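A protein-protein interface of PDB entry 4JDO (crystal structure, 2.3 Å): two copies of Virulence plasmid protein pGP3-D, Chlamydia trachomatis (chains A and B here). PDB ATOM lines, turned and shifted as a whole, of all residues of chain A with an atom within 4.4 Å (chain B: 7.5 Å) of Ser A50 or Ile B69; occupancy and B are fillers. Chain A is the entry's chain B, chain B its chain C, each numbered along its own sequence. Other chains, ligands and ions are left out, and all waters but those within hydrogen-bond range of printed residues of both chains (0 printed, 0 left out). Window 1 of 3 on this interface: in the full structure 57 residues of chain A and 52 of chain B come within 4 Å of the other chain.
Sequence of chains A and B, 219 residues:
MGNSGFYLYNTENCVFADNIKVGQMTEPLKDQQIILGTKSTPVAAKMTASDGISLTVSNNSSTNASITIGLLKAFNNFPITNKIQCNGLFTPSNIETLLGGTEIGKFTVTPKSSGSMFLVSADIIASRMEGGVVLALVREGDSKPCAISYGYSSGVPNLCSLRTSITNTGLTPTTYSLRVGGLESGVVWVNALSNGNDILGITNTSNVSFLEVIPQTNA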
ATOM      1  N   MET A  47       5.526  14.728   3.344  1.00  0.00           N
ATOM      2  CA  MET A  47       6.292  13.494   3.403  1.00  0.00           C
ATOM      3  C   MET A  47       6.256  12.837   2.042  1.00  0.00           C
ATOM      4  O   MET A  47       5.190  12.736   1.440  1.00  0.00           O
ATOM      5  CB  MET A  47       5.725  12.541   4.451  1.00  0.00           C
ATOM      6  CG  MET A  47       5.848  13.046   5.878  1.00  0.00           C
ATOM      7  SD  MET A  47       5.708  11.623   7.207  1.00  0.00           S
ATOM      8  CE  MET A  47       7.436  10.775   6.904  1.00  0.00           C
ATOM      9  N   THR A  48       7.420  12.421   1.544  1.00  0.00           N
ATOM     10  CA  THR A  48       7.485  11.658   0.303  1.00  0.00           C
ATOM     11  C   THR A  48       8.490  10.526   0.389  1.00  0.00           C
ATOM     12  O   THR A  48       9.454  10.589   1.155  1.00  0.00           O
ATOM     13  CB  THR A  48       7.825  12.532  -0.933  1.00  0.00           C
ATOM     14  OG1 THR A  48       9.077  13.198  -0.738  1.00  0.00           O
ATOM     15  CG2 THR A  48       6.740  13.560  -1.170  1.00  0.00           C
ATOM     16  N   ALA A  49       8.259   9.491  -0.409  1.00  0.00           N
ATOM     17  CA  ALA A  49       9.179   8.367  -0.488  1.00  0.00           C
ATOM     18  C   ALA A  49      10.036   8.453  -1.734  1.00  0.00           C
ATOM     19  O   ALA A  49       9.723   9.187  -2.662  1.00  0.00           O
ATOM     20  CB  ALA A  49       8.413   7.072  -0.489  1.00  0.00           C
ATOM     21  N   SER A  50      11.123   7.693  -1.728  1.00  0.00           N
ATOM     22  CA  SER A  50      11.960   7.472  -2.899  1.00  0.00           C
ATOM     23  C   SER A  50      12.781   6.227  -2.590  1.00  0.00           C
ATOM     24  O   SER A  50      12.611   5.639  -1.519  1.00  0.00           O
ATOM     25  CB  SER A  50      12.885   8.659  -3.125  1.00  0.00           C
ATOM     26  OG  SER A  50      13.757   8.815  -2.021  1.00  0.00           O
ATOM     27  N   ASP A  51      13.658   5.830  -3.515  1.00  0.00           N
ATOM     28  CA  ASP A  51      14.602   4.727  -3.290  1.00  0.00           C
ATOM     29  C   ASP A  51      13.987   3.493  -2.629  1.00  0.00           C
ATOM     30  O   ASP A  51      14.374   3.136  -1.517  1.00  0.00           O
ATOM     31  CB  ASP A  51      15.771   5.191  -2.409  1.00  0.00           C
ATOM     32  CG  ASP A  51      16.808   5.991  -3.170  1.00  0.00           C
ATOM     33  OD1 ASP A  51      16.506   6.446  -4.299  1.00  0.00           O
ATOM     34  OD2 ASP A  51      17.929   6.166  -2.630  1.00  0.00           O
ATOM     35  N   GLY A  52      13.034   2.847  -3.289  1.00  0.00           N
ATOM     36  CA  GLY A  52      12.490   1.606  -2.765  1.00  0.00           C
ATOM     37  C   GLY A  52      11.660   1.739  -1.504  1.00  0.00           C
ATOM     38  O   GLY A  52      11.520   0.775  -0.758  1.00  0.00           O
ATOM     39  N   ILE A  53      11.114   2.931  -1.260  1.00  0.00           N
ATOM     40  CA  ILE A  53      10.232   3.154  -0.108  1.00  0.00           C
ATOM     41  C   ILE A  53       8.802   3.451  -0.559  1.00  0.00           C
ATOM     42  O   ILE A  53       8.577   4.191  -1.514  1.00  0.00           O
ATOM     43  CB  ILE A  53      10.741   4.292   0.819  1.00  0.00           C
ATOM     44  CG1 ILE A  53      12.047   3.887   1.512  1.00  0.00           C
ATOM     45  CG2 ILE A  53       9.710   4.635   1.882  1.00  0.00           C
ATOM     46  CD1 ILE A  53      11.884   2.768   2.508  1.00  0.00           C
ATOM     47  N   MET B  47      12.213  13.697  14.660  1.00  0.00           N
ATOM     48  CA  MET B  47      12.073  12.626  13.686  1.00  0.00           C
ATOM     49  C   MET B  47      13.409  12.300  13.013  1.00  0.00           C
ATOM     50  O   MET B  47      14.036  13.172  12.437  1.00  0.00           O
ATOM     51  CB  MET B  47      11.019  12.999  12.646  1.00  0.00           C
ATOM     52  CG  MET B  47      10.759  11.883  11.653  1.00  0.00           C
ATOM     53  SD  MET B  47       9.041  12.047  10.740  1.00  0.00           S
ATOM     54  CE  MET B  47       9.279  13.811   9.978  1.00  0.00           C
ATOM     55  N   THR B  48      13.842  11.046  13.095  1.00  0.00           N
ATOM     56  CA  THR B  48      15.168  10.648  12.608  1.00  0.00           C
ATOM     57  C   THR B  48      15.187   9.272  11.965  1.00  0.00           C
ATOM     58  O   THR B  48      14.358   8.413  12.264  1.00  0.00           O
ATOM     59  CB  THR B  48      16.223  10.615  13.734  1.00  0.00           C
ATOM     60  OG1 THR B  48      15.704   9.892  14.860  1.00  0.00           O
ATOM     61  CG2 THR B  48      16.618  12.035  14.161  1.00  0.00           C
ATOM     62  N   ALA B  49      16.159   9.065  11.086  1.00  0.00           N
ATOM     63  CA  ALA B  49      16.327   7.780  10.439  1.00  0.00           C
ATOM     64  C   ALA B  49      17.436   7.013  11.130  1.00  0.00           C
ATOM     65  O   ALA B  49      18.191   7.575  11.919  1.00  0.00           O
ATOM     66  CB  ALA B  49      16.659   7.976   8.986  1.00  0.00           C
ATOM     67  N   ILE B  53      18.059   3.568   6.612  1.00  0.00           N
ATOM     68  CA  ILE B  53      17.144   4.596   6.103  1.00  0.00           C
ATOM     69  C   ILE B  53      17.810   5.969   6.110  1.00  0.00           C
ATOM     70  O   ILE B  53      18.497   6.326   7.066  1.00  0.00           O
ATOM     71  CB  ILE B  53      15.844   4.674   6.937  1.00  0.00           C
ATOM     72  CG1 ILE B  53      15.169   3.311   6.986  1.00  0.00           C
ATOM     73  CG2 ILE B  53      14.887   5.715   6.354  1.00  0.00           C
ATOM     74  CD1 ILE B  53      14.605   2.881   5.657  1.00  0.00           C
ATOM     75  N   SER B  54      17.625   6.727   5.036  1.00  0.00           N
ATOM     76  CA  SER B  54      17.965   8.144   5.070  1.00  0.00           C
ATOM     77  C   SER B  54      16.719   9.013   5.253  1.00  0.00           C
ATOM     78  O   SER B  54      15.657   8.747   4.683  1.00  0.00           O
ATOM     79  CB  SER B  54      18.702   8.581   3.809  1.00  0.00           C
ATOM     80  OG  SER B  54      17.819   8.611   2.705  1.00  0.00           O
ATOM     81  N   LEU B  55      16.873  10.062   6.047  1.00  0.00           N
ATOM     82  CA  LEU B  55      15.821  11.041   6.239  1.00  0.00           C
ATOM     83  C   LEU B  55      16.326  12.378   5.724  1.00  0.00           C
ATOM     84  O   LEU B  55      17.348  12.880   6.198  1.00  0.00           O
ATOM     85  CB  LEU B  55      15.475  11.132   7.724  1.00  0.00           C
ATOM     86  CG  LEU B  55      13.984  10.982   7.993  1.00  0.00           C
ATOM     87  CD1 LEU B  55      13.675  10.815   9.446  1.00  0.00           C
ATOM     88  CD2 LEU B  55      13.342  12.205   7.481  1.00  0.00           C
ATOM     89  N   THR B  56      15.616  12.955   4.757  1.00  0.00           N
ATOM     90  CA  THR B  56      16.115  14.147   4.069  1.00  0.00           C
ATOM     91  C   THR B  56      15.103  15.294   3.954  1.00  0.00           C
ATOM     92  O   THR B  56      14.041  15.146   3.354  1.00  0.00           O
ATOM     93  CB  THR B  56      16.713  13.774   2.678  1.00  0.00           C
ATOM     94  OG1 THR B  56      18.058  13.320   2.860  1.00  0.00           O
ATOM     95  CG2 THR B  56      16.728  14.972   1.729  1.00  0.00           C
ATOM     96  N   SER B  66       9.816  19.744   2.074  1.00  0.00           N
ATOM     97  CA  SER B  66       9.712  18.334   1.756  1.00  0.00           C
ATOM     98  C   SER B  66      10.545  17.502   2.710  1.00  0.00           C
ATOM     99  O   SER B  66      11.624  17.905   3.142  1.00  0.00           O
ATOM    100  CB  SER B  66      10.159  18.097   0.307  1.00  0.00           C
ATOM    101  OG  SER B  66       9.773  16.813  -0.142  1.00  0.00           O
ATOM    102  N   ILE B  67      10.030  16.334   3.053  1.00  0.00           N
ATOM    103  CA  ILE B  67      10.788  15.395   3.855  1.00  0.00           C
ATOM    104  C   ILE B  67      10.757  14.045   3.136  1.00  0.00           C
ATOM    105  O   ILE B  67       9.692  13.468   2.908  1.00  0.00           O
ATOM    106  CB  ILE B  67      10.279  15.366   5.318  1.00  0.00           C
ATOM    107  CG1 ILE B  67      11.100  14.415   6.168  1.00  0.00           C
ATOM    108  CG2 ILE B  67       8.802  15.051   5.395  1.00  0.00           C
ATOM    109  CD1 ILE B  67      11.422  15.001   7.532  1.00  0.00           C
ATOM    110  N   THR B  68      11.933  13.588   2.715  1.00  0.00           N
ATOM    111  CA  THR B  68      12.050  12.406   1.871  1.00  0.00           C
ATOM    112  C   THR B  68      12.559  11.222   2.662  1.00  0.00           C
ATOM    113  O   THR B  68      13.626  11.290   3.256  1.00  0.00           O
ATOM    114  CB  THR B  68      13.058  12.624   0.719  1.00  0.00           C
ATOM    115  OG1 THR B  68      12.763  13.847   0.039  1.00  0.00           O
ATOM    116  CG2 THR B  68      12.998  11.464  -0.280  1.00  0.00           C
ATOM    117  N   ILE B  69      11.804  10.133   2.660  1.00  0.00           N
ATOM    118  CA  ILE B  69      12.294   8.892   3.238  1.00  0.00           C
ATOM    119  C   ILE B  69      12.809   8.013   2.110  1.00  0.00           C
ATOM    120  O   ILE B  69      12.156   7.905   1.073  1.00  0.00           O
ATOM    121  CB  ILE B  69      11.186   8.123   3.954  1.00  0.00           C
ATOM    122  CG1 ILE B  69      10.433   9.046   4.916  1.00  0.00           C
ATOM    123  CG2 ILE B  69      11.765   6.903   4.669  1.00  0.00           C
ATOM    124  CD1 ILE B  69      11.325   9.756   5.877  1.00  0.00           C
ATOM    125  N   GLY B  70      13.973   7.397   2.305  1.00  0.00           N
ATOM    126  CA  GLY B  70      14.519   6.480   1.316  1.00  0.00           C
ATOM    127  C   GLY B  70      15.539   5.488   1.843  1.00  0.00           C
ATOM    128  O   GLY B  70      16.056   5.637   2.948  1.00  0.00           O
ATOM    129  N   LEU B  71      15.834   4.465   1.048  1.00  0.00           N
ATOM    130  CA  LEU B  71      16.840   3.475   1.427  1.00  0.00           C
ATOM    131  C   LEU B  71      18.243   4.012   1.213  1.00  0.00           C
ATOM    132  O   LEU B  71      18.530   4.615   0.191  1.00  0.00           O
ATOM    133  CB  LEU B  71      16.690   2.208   0.594  1.00  0.00           C
ATOM    134  CG  LEU B  71      15.567   1.229   0.920  1.00  0.00           C
ATOM    135  CD1 LEU B  71      15.631   0.039  -0.030  1.00  0.00           C
ATOM    136  CD2 LEU B  71      15.689   0.785   2.358  1.00  0.00           C
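Met A47 touches Ile B67 (CA to O, 3.4 Å).
Ile B69 touches Met A47 (CG1 to CE, 3.99 Å).
OG1 of Thr A48 touches OG of Ser B66, 3.7 Å away.
Thr A48 touches Thr B68.
Ala A49 touches Ile B69.
Ser A50 touches Thr B68 (OG to CG2, 3.3 Å).
Ser A50 touches Gly B70.
CB of Ile A53 touches O of Ile B69, at 3.9 Å.
CG1 of Ile A53 touches CA of Gly B70, 3.6 Å away.
Leu B71 touches Ile A53 (N to CG1, 3.9 Å).
Along chain A the printed residues that touch a printed residue of chain B span positions 47 to 53.
Among the printed residues, 14 pairs touch across the chains.
N of Ser B54 sits at hydrogen-bond distance from O of Gly B70 (2.8 Å).
The backbone carbonyl oxygen (O) of Thr B56 is in hydrogen-bond range of the backbone NH (N) of Thr B68 (2.7 Å).
Of the printed residues of chain B, Ser A50 touches Thr B68 (3.3 Å), Ile B69 (3.0 Å) and Gly B70 (3.5 Å).
Of the printed residues of chain A, Ile B69 touches Met A47, Thr A48, Ala A49, Ser A50 and Ile A53.
Printed residues of chain B within 4 Å of Asp A51: Leu B71 (3.2 Å).
Of the printed residues of chain A, Ile B67 touches Met A47 (3.4 Å) and Thr A48 (2.8 Å).
Of the printed residues of chain A, Leu B71 touches Asp A51 and Ile A53.
Leu B55 touches none of the printed residues of chain A.
The nearest printed residue of chain A that does not touch Ile B69 is Asp A51 (5.3 Å).
The nearest printed residue of chain B that does not touch Thr A48 is Gly B70 (5.7 Å).
Positions printed for both chains: 47, 48, 49 and 53.
Of the 14 pairs that touch across the chains among the printed residues, none has its exchanged pair printed and touching as well.
N of Thr A48 is in hydrogen-bond range of O of Ile B67.
The backbone carbonyl oxygen (O) of Thr A48 lies within hydrogen-bond range of the backbone NH (N) of Ile B69.
N of Ser A50 lies within hydrogen-bond range of O of Ile B69.
N of Leu B71 sits at hydrogen-bond distance from O of Asp A51, at 3.2 Å.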
